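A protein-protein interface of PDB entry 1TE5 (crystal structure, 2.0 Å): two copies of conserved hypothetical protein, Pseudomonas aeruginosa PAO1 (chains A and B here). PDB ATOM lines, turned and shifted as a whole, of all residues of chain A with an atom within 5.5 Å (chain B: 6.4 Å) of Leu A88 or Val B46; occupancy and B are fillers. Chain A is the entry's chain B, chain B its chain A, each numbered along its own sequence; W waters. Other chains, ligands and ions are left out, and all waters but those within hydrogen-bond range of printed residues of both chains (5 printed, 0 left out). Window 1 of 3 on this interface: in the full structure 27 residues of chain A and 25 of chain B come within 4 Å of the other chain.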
ATOM      1  N   GLN A  50     -10.302  11.673  26.082  1.00  0.00           N
ATOM      2  CA  GLN A  50     -10.034  12.383  27.312  1.00  0.00           C
ATOM      3  C   GLN A  50      -9.375  11.422  28.293  1.00  0.00           C
ATOM      4  O   GLN A  50      -9.562  10.211  28.198  1.00  0.00           O
ATOM      5  CB  GLN A  50     -11.336  13.001  27.841  1.00  0.00           C
ATOM      6  CG  GLN A  50     -11.803  14.177  26.970  1.00  0.00           C
ATOM      7  CD  GLN A  50     -13.302  14.293  26.867  1.00  0.00           C
ATOM      8  OE1 GLN A  50     -13.850  15.387  26.989  1.00  0.00           O
ATOM      9  NE2 GLN A  50     -13.978  13.171  26.600  1.00  0.00           N
ATOM     10  N   VAL A  83      -9.727  13.789  35.199  1.00  0.00           N
ATOM     11  CA  VAL A  83     -11.171  13.701  34.986  1.00  0.00           C
ATOM     12  C   VAL A  83     -11.923  13.309  36.274  1.00  0.00           C
ATOM     13  O   VAL A  83     -13.131  13.509  36.393  1.00  0.00           O
ATOM     14  CB  VAL A  83     -11.506  12.724  33.815  1.00  0.00           C
ATOM     15  CG1 VAL A  83     -11.856  11.329  34.328  1.00  0.00           C
ATOM     16  CG2 VAL A  83     -12.619  13.289  32.959  1.00  0.00           C
ATOM     17  N   VAL A  86     -12.458  17.049  38.023  1.00  0.00           N
ATOM     18  CA  VAL A  86     -13.428  17.977  37.437  1.00  0.00           C
ATOM     19  C   VAL A  86     -14.630  17.280  36.835  1.00  0.00           C
ATOM     20  O   VAL A  86     -15.675  17.898  36.668  1.00  0.00           O
ATOM     21  CB  VAL A  86     -12.823  18.886  36.337  1.00  0.00           C
ATOM     22  CG1 VAL A  86     -11.832  19.866  36.942  1.00  0.00           C
ATOM     23  CG2 VAL A  86     -12.182  18.046  35.229  1.00  0.00           C
ATOM     24  N   GLY A  87     -14.478  15.997  36.518  1.00  0.00           N
ATOM     25  CA  GLY A  87     -15.559  15.236  35.914  1.00  0.00           C
ATOM     26  C   GLY A  87     -15.470  15.264  34.398  1.00  0.00           C
ATOM     27  O   GLY A  87     -14.930  16.201  33.814  1.00  0.00           O
ATOM     28  N   LEU A  88     -16.005  14.238  33.750  1.00  0.00           N
ATOM     29  CA  LEU A  88     -15.972  14.170  32.298  1.00  0.00           C
ATOM     30  C   LEU A  88     -16.744  15.297  31.590  1.00  0.00           C
ATOM     31  O   LEU A  88     -16.308  15.791  30.548  1.00  0.00           O
ATOM     32  CB  LEU A  88     -16.485  12.807  31.829  1.00  0.00           C
ATOM     33  CG  LEU A  88     -16.416  12.516  30.326  1.00  0.00           C
ATOM     34  CD1 LEU A  88     -14.967  12.492  29.859  1.00  0.00           C
ATOM     35  CD2 LEU A  88     -17.090  11.195  30.027  1.00  0.00           C
ATOM     36  N   SER A  89     -17.920  15.649  32.108  1.00  0.00           N
ATOM     37  CA  SER A  89     -18.724  16.716  31.502  1.00  0.00           C
ATOM     38  C   SER A  89     -18.046  18.086  31.538  1.00  0.00           C
ATOM     39  O   SER A  89     -18.435  18.993  30.792  1.00  0.00           O
ATOM     40  CB  SER A  89     -20.119  16.795  32.152  1.00  0.00           C
ATOM     41  OG  SER A  89     -20.068  16.901  33.569  1.00  0.00           O
ATOM     42  N   ASN A  90     -17.010  18.216  32.364  1.00  0.00           N
ATOM     43  CA  ASN A  90     -16.281  19.475  32.510  1.00  0.00           C
ATOM     44  C   ASN A  90     -14.892  19.453  31.893  1.00  0.00           C
ATOM     45  O   ASN A  90     -14.067  20.318  32.192  1.00  0.00           O
ATOM     46  CB  ASN A  90     -16.211  19.847  33.987  1.00  0.00           C
ATOM     47  CG  ASN A  90     -17.573  19.950  34.605  1.00  0.00           C
ATOM     48  OD1 ASN A  90     -18.476  20.570  34.051  1.00  0.00           O
ATOM     49  ND2 ASN A  90     -17.730  19.355  35.777  1.00  0.00           N
ATOM     50  N   THR A  91     -14.649  18.477  31.021  1.00  0.00           N
ATOM     51  CA  THR A  91     -13.356  18.340  30.357  1.00  0.00           C
ATOM     52  C   THR A  91     -13.393  18.842  28.904  1.00  0.00           C
ATOM     53  O   THR A  91     -14.352  18.601  28.165  1.00  0.00           O
ATOM     54  CB  THR A  91     -12.853  16.868  30.388  1.00  0.00           C
ATOM     55  OG1 THR A  91     -12.921  16.358  31.725  1.00  0.00           O
ATOM     56  CG2 THR A  91     -11.403  16.794  29.945  1.00  0.00           C
ATOM     57  N   ALA B  39     -20.544   3.847  22.942  1.00  0.00           N
ATOM     58  CA  ALA B  39     -20.667   5.080  23.697  1.00  0.00           C
ATOM     59  C   ALA B  39     -21.151   4.699  25.080  1.00  0.00           C
ATOM     60  O   ALA B  39     -21.902   3.746  25.234  1.00  0.00           O
ATOM     61  CB  ALA B  39     -21.654   6.009  23.031  1.00  0.00           C
ATOM     62  N   PHE B  40     -20.635   5.375  26.094  1.00  0.00           N
ATOM     63  CA  PHE B  40     -21.053   5.115  27.461  1.00  0.00           C
ATOM     64  C   PHE B  40     -20.932   6.378  28.299  1.00  0.00           C
ATOM     65  O   PHE B  40     -20.252   7.325  27.906  1.00  0.00           O
ATOM     66  CB  PHE B  40     -20.289   3.934  28.077  1.00  0.00           C
ATOM     67  CG  PHE B  40     -18.808   4.124  28.144  1.00  0.00           C
ATOM     68  CD1 PHE B  40     -18.203   4.590  29.315  1.00  0.00           C
ATOM     69  CD2 PHE B  40     -18.006   3.802  27.051  1.00  0.00           C
ATOM     70  CE1 PHE B  40     -16.810   4.733  29.402  1.00  0.00           C
ATOM     71  CE2 PHE B  40     -16.618   3.940  27.118  1.00  0.00           C
ATOM     72  CZ  PHE B  40     -16.018   4.406  28.299  1.00  0.00           C
ATOM     73  N   TYR B  41     -21.609   6.403  29.441  1.00  0.00           N
ATOM     74  CA  TYR B  41     -21.599   7.581  30.290  1.00  0.00           C
ATOM     75  C   TYR B  41     -20.805   7.504  31.574  1.00  0.00           C
ATOM     76  O   TYR B  41     -20.693   6.459  32.191  1.00  0.00           O
ATOM     77  CB  TYR B  41     -23.033   7.985  30.606  1.00  0.00           C
ATOM     78  CG  TYR B  41     -23.824   8.325  29.375  1.00  0.00           C
ATOM     79  CD1 TYR B  41     -24.321   7.321  28.546  1.00  0.00           C
ATOM     80  CD2 TYR B  41     -24.074   9.648  29.037  1.00  0.00           C
ATOM     81  CE1 TYR B  41     -25.047   7.627  27.406  1.00  0.00           C
ATOM     82  CE2 TYR B  41     -24.798   9.968  27.902  1.00  0.00           C
ATOM     83  CZ  TYR B  41     -25.283   8.957  27.092  1.00  0.00           C
ATOM     84  OH  TYR B  41     -25.997   9.283  25.970  1.00  0.00           O
ATOM     85  N   GLU B  42     -20.292   8.655  31.985  1.00  0.00           N
ATOM     86  CA  GLU B  42     -19.519   8.816  33.206  1.00  0.00           C
ATOM     87  C   GLU B  42     -20.073  10.066  33.882  1.00  0.00           C
ATOM     88  O   GLU B  42     -19.487  11.152  33.887  1.00  0.00           O
ATOM     89  CB  GLU B  42     -18.063   9.075  32.835  1.00  0.00           C
ATOM     90  CG  GLU B  42     -17.041   8.445  33.751  1.00  0.00           C
ATOM     91  CD  GLU B  42     -15.676   8.323  33.085  1.00  0.00           C
ATOM     92  OE1 GLU B  42     -15.491   7.388  32.272  1.00  0.00           O
ATOM     93  OE2 GLU B  42     -14.793   9.159  33.376  1.00  0.00           O
ATOM     94  N   GLY B  43     -21.276   9.884  34.423  1.00  0.00           N
ATOM     95  CA  GLY B  43     -22.004  10.996  35.001  1.00  0.00           C
ATOM     96  C   GLY B  43     -22.854  11.523  33.841  1.00  0.00           C
ATOM     97  O   GLY B  43     -23.566  10.728  33.213  1.00  0.00           O
ATOM     98  N   ARG B  44     -22.797  12.821  33.556  1.00  0.00           N
ATOM     99  CA  ARG B  44     -23.538  13.364  32.422  1.00  0.00           C
ATOM    100  C   ARG B  44     -22.668  13.340  31.179  1.00  0.00           C
ATOM    101  O   ARG B  44     -23.167  13.482  30.066  1.00  0.00           O
ATOM    102  CB  ARG B  44     -24.041  14.780  32.705  1.00  0.00           C
ATOM    103  CG  ARG B  44     -25.242  14.786  33.630  1.00  0.00           C
ATOM    104  CD  ARG B  44     -25.653  16.179  34.057  1.00  0.00           C
ATOM    105  NE  ARG B  44     -26.373  16.118  35.327  1.00  0.00           N
ATOM    106  CZ  ARG B  44     -27.527  16.725  35.576  1.00  0.00           C
ATOM    107  NH1 ARG B  44     -28.086  16.589  36.770  1.00  0.00           N
ATOM    108  NH2 ARG B  44     -28.113  17.473  34.646  1.00  0.00           N
ATOM    109  N   GLY B  45     -21.365  13.175  31.383  1.00  0.00           N
ATOM    110  CA  GLY B  45     -20.424  13.113  30.280  1.00  0.00           C
ATOM    111  C   GLY B  45     -20.514  11.797  29.523  1.00  0.00           C
ATOM    112  O   GLY B  45     -20.919  10.788  30.082  1.00  0.00           O
ATOM    113  N   VAL B  46     -20.128  11.806  28.251  1.00  0.00           N
ATOM    114  CA  VAL B  46     -20.186  10.603  27.422  1.00  0.00           C
ATOM    115  C   VAL B  46     -18.871  10.344  26.692  1.00  0.00           C
ATOM    116  O   VAL B  46     -18.188  11.279  26.261  1.00  0.00           O
ATOM    117  CB  VAL B  46     -21.349  10.691  26.385  1.00  0.00           C
ATOM    118  CG1 VAL B  46     -21.215  11.926  25.538  1.00  0.00           C
ATOM    119  CG2 VAL B  46     -21.363   9.477  25.488  1.00  0.00           C
ATOM    120  N   ARG B  47     -18.480   9.077  26.617  1.00  0.00           N
ATOM    121  CA  ARG B  47     -17.265   8.688  25.907  1.00  0.00           C
ATOM    122  C   ARG B  47     -17.667   7.936  24.644  1.00  0.00           C
ATOM    123  O   ARG B  47     -18.564   7.105  24.672  1.00  0.00           O
ATOM    124  CB  ARG B  47     -16.377   7.801  26.777  1.00  0.00           C
ATOM    125  CG  ARG B  47     -15.820   8.493  27.998  1.00  0.00           C
ATOM    126  CD  ARG B  47     -14.763   7.641  28.648  1.00  0.00           C
ATOM    127  NE  ARG B  47     -14.279   8.201  29.905  1.00  0.00           N
ATOM    128  CZ  ARG B  47     -13.242   9.026  30.020  1.00  0.00           C
ATOM    129  NH1 ARG B  47     -12.886   9.472  31.213  1.00  0.00           N
ATOM    130  NH2 ARG B  47     -12.564   9.407  28.941  1.00  0.00           N
ATOM    131  N   LEU B  48     -17.003   8.228  23.536  1.00  0.00           N
ATOM    132  CA  LEU B  48     -17.323   7.577  22.277  1.00  0.00           C
ATOM    133  C   LEU B  48     -16.085   7.037  21.561  1.00  0.00           C
ATOM    134  O   LEU B  48     -15.118   7.769  21.319  1.00  0.00           O
ATOM    135  CB  LEU B  48     -18.061   8.552  21.354  1.00  0.00           C
ATOM    136  CG  LEU B  48     -18.452   8.053  19.958  1.00  0.00           C
ATOM    137  CD1 LEU B  48     -19.482   6.927  20.051  1.00  0.00           C
ATOM    138  CD2 LEU B  48     -18.991   9.214  19.150  1.00  0.00           C
ATOM    139  N   ILE B  95     -24.115  11.176  18.552  1.00  0.00           N
ATOM    140  CA  ILE B  95     -24.352  11.994  19.741  1.00  0.00           C
ATOM    141  C   ILE B  95     -24.781  13.415  19.383  1.00  0.00           C
ATOM    142  O   ILE B  95     -24.330  13.982  18.387  1.00  0.00           O
ATOM    143  CB  ILE B  95     -23.084  12.083  20.624  1.00  0.00           C
ATOM    144  CG1 ILE B  95     -22.540  10.685  20.921  1.00  0.00           C
ATOM    145  CG2 ILE B  95     -23.382  12.829  21.929  1.00  0.00           C
ATOM    146  CD1 ILE B  95     -21.315  10.700  21.782  1.00  0.00           C
ATOM    147  N   TYR B 102     -26.417  14.843  26.827  1.00  0.00           N
ATOM    148  CA  TYR B 102     -25.904  14.297  25.569  1.00  0.00           C
ATOM    149  C   TYR B 102     -26.785  13.121  25.182  1.00  0.00           C
ATOM    150  O   TYR B 102     -27.005  12.224  25.981  1.00  0.00           O
ATOM    151  CB  TYR B 102     -24.441  13.845  25.702  1.00  0.00           C
ATOM    152  CG  TYR B 102     -23.430  14.977  25.773  1.00  0.00           C
ATOM    153  CD1 TYR B 102     -22.606  15.131  26.891  1.00  0.00           C
ATOM    154  CD2 TYR B 102     -23.295  15.905  24.727  1.00  0.00           C
ATOM    155  CE1 TYR B 102     -21.690  16.171  26.973  1.00  0.00           C
ATOM    156  CE2 TYR B 102     -22.378  16.955  24.809  1.00  0.00           C
ATOM    157  CZ  TYR B 102     -21.585  17.075  25.931  1.00  0.00           C
ATOM    158  OH  TYR B 102     -20.698  18.122  26.036  1.00  0.00           O
ATOM    159  N   THR B 104     -27.608   9.826  22.851  1.00  0.00           N
ATOM    160  CA  THR B 104     -26.885   8.809  22.087  1.00  0.00           C
ATOM    161  C   THR B 104     -27.903   7.973  21.302  1.00  0.00           C
ATOM    162  O   THR B 104     -28.953   7.610  21.830  1.00  0.00           O
ATOM    163  CB  THR B 104     -26.020   7.922  23.028  1.00  0.00           C
ATOM    164  OG1 THR B 104     -24.959   8.706  23.599  1.00  0.00           O
ATOM    165  CG2 THR B 104     -25.396   6.777  22.259  1.00  0.00           C
HETATM  166  O   HOH W   1     -12.084   8.856  25.538  1.00  0.00           O
HETATM  167  O   HOH W   2     -21.452  14.632  35.268  1.00  0.00           O
HETATM  168  O   HOH W   3     -15.829  11.356  34.891  1.00  0.00           O
HETATM  169  O   HOH W   4     -19.081  14.172  34.143  1.00  0.00           O
HETATM  170  O   HOH W   5     -19.756  18.561  28.503  1.00  0.00           O
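The guanidinium group (NH2) of Arg B47 sits at hydrogen-bond distance from the backbone carbonyl oxygen (O) of Gln A50.
CG1 of Val A83 touches OE2 of Glu B42, 3.8 Å away.
Val A83 touches Arg B47 (CG1 to NH1, 3.8 Å).
Glu B42 touches Leu A88 (CB to CD2, 3.7 Å).
Leu A88 touches Gly B45 (CD2 to C, 3.5 Å).
Leu A88 touches Val B46 (CD2 to N, 3.6 Å).
Leu A88 touches Arg B47 (CD2 to CG, 3.6 Å).
CB of Ser A89 touches N of Gly B45 (3.9 Å).
No position is printed for both chains.
Of the 8 pairs that touch across the chains among the printed residues, none has its exchanged pair printed and touching as well.
Of the 8 printed residues of chain A, 4 touch a printed residue of chain B.
Printed residues of chain A that touch a printed residue of chain B: Gln A50, Val A83, Leu A88 and Ser A89.
Hydrophobic or aromatic side chains of chain A that line the printed part of chain B: Val A83 and Leu A88.
Along chain A the printed residues that touch a printed residue of chain B span positions 50 to 89.
Among the printed residues, 8 pairs touch across the chains.
Of chain B, only Glu B42, Gly B45, Val B46 and Arg B47 come within 4 Å of Leu A88.
Printed residues of chain A within 4 Å of Val B46: Leu A88 (3.6 Å).
Printed residues of chain A within 4 Å of Glu B42: Val A83 and Leu A88.
Of the printed residues of chain B, Val A83 touches Glu B42 (3.8 Å) and Arg B47 (3.8 Å).
The nearest residue of chain B that does not touch Leu A88 is Phe B40 (5.4 Å).
N of Arg B47 is in hydrogen-bond range of O of Phe B40.
The backbone carbonyl oxygen (O) of Thr A91 sits close to the side-chain amide oxygen (OE1) of Gln A50 (3.5 Å).
NE of Arg B47 lies within salt-bridge range of OE1 of Glu B42 (2.8 Å).
Water W5 bridges the side-chain hydroxyl (OH) of Tyr B102 (2.7 Å) and the backbone carbonyl oxygen (O) of Ser A89 (2.7 Å).
Water W4 lies within hydrogen-bond range of N of Ser A89 (2.8 Å), O of Glu B42 (3.1 Å) and N of Leu A88 (3.1 Å).
Water W2 bridges the backbone NH of Arg B44 (2.8 Å) and the side-chain hydroxyl of Ser A89 (3.2 Å).
Water W3 bridges the side-chain carboxylate (OE2) of Glu B42 and the backbone NH (N) of Leu A88.
Water W1 lies within hydrogen-bond range of the backbone NH (N) of Gln A50 and the guanidinium group (NH2) of Arg B47.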
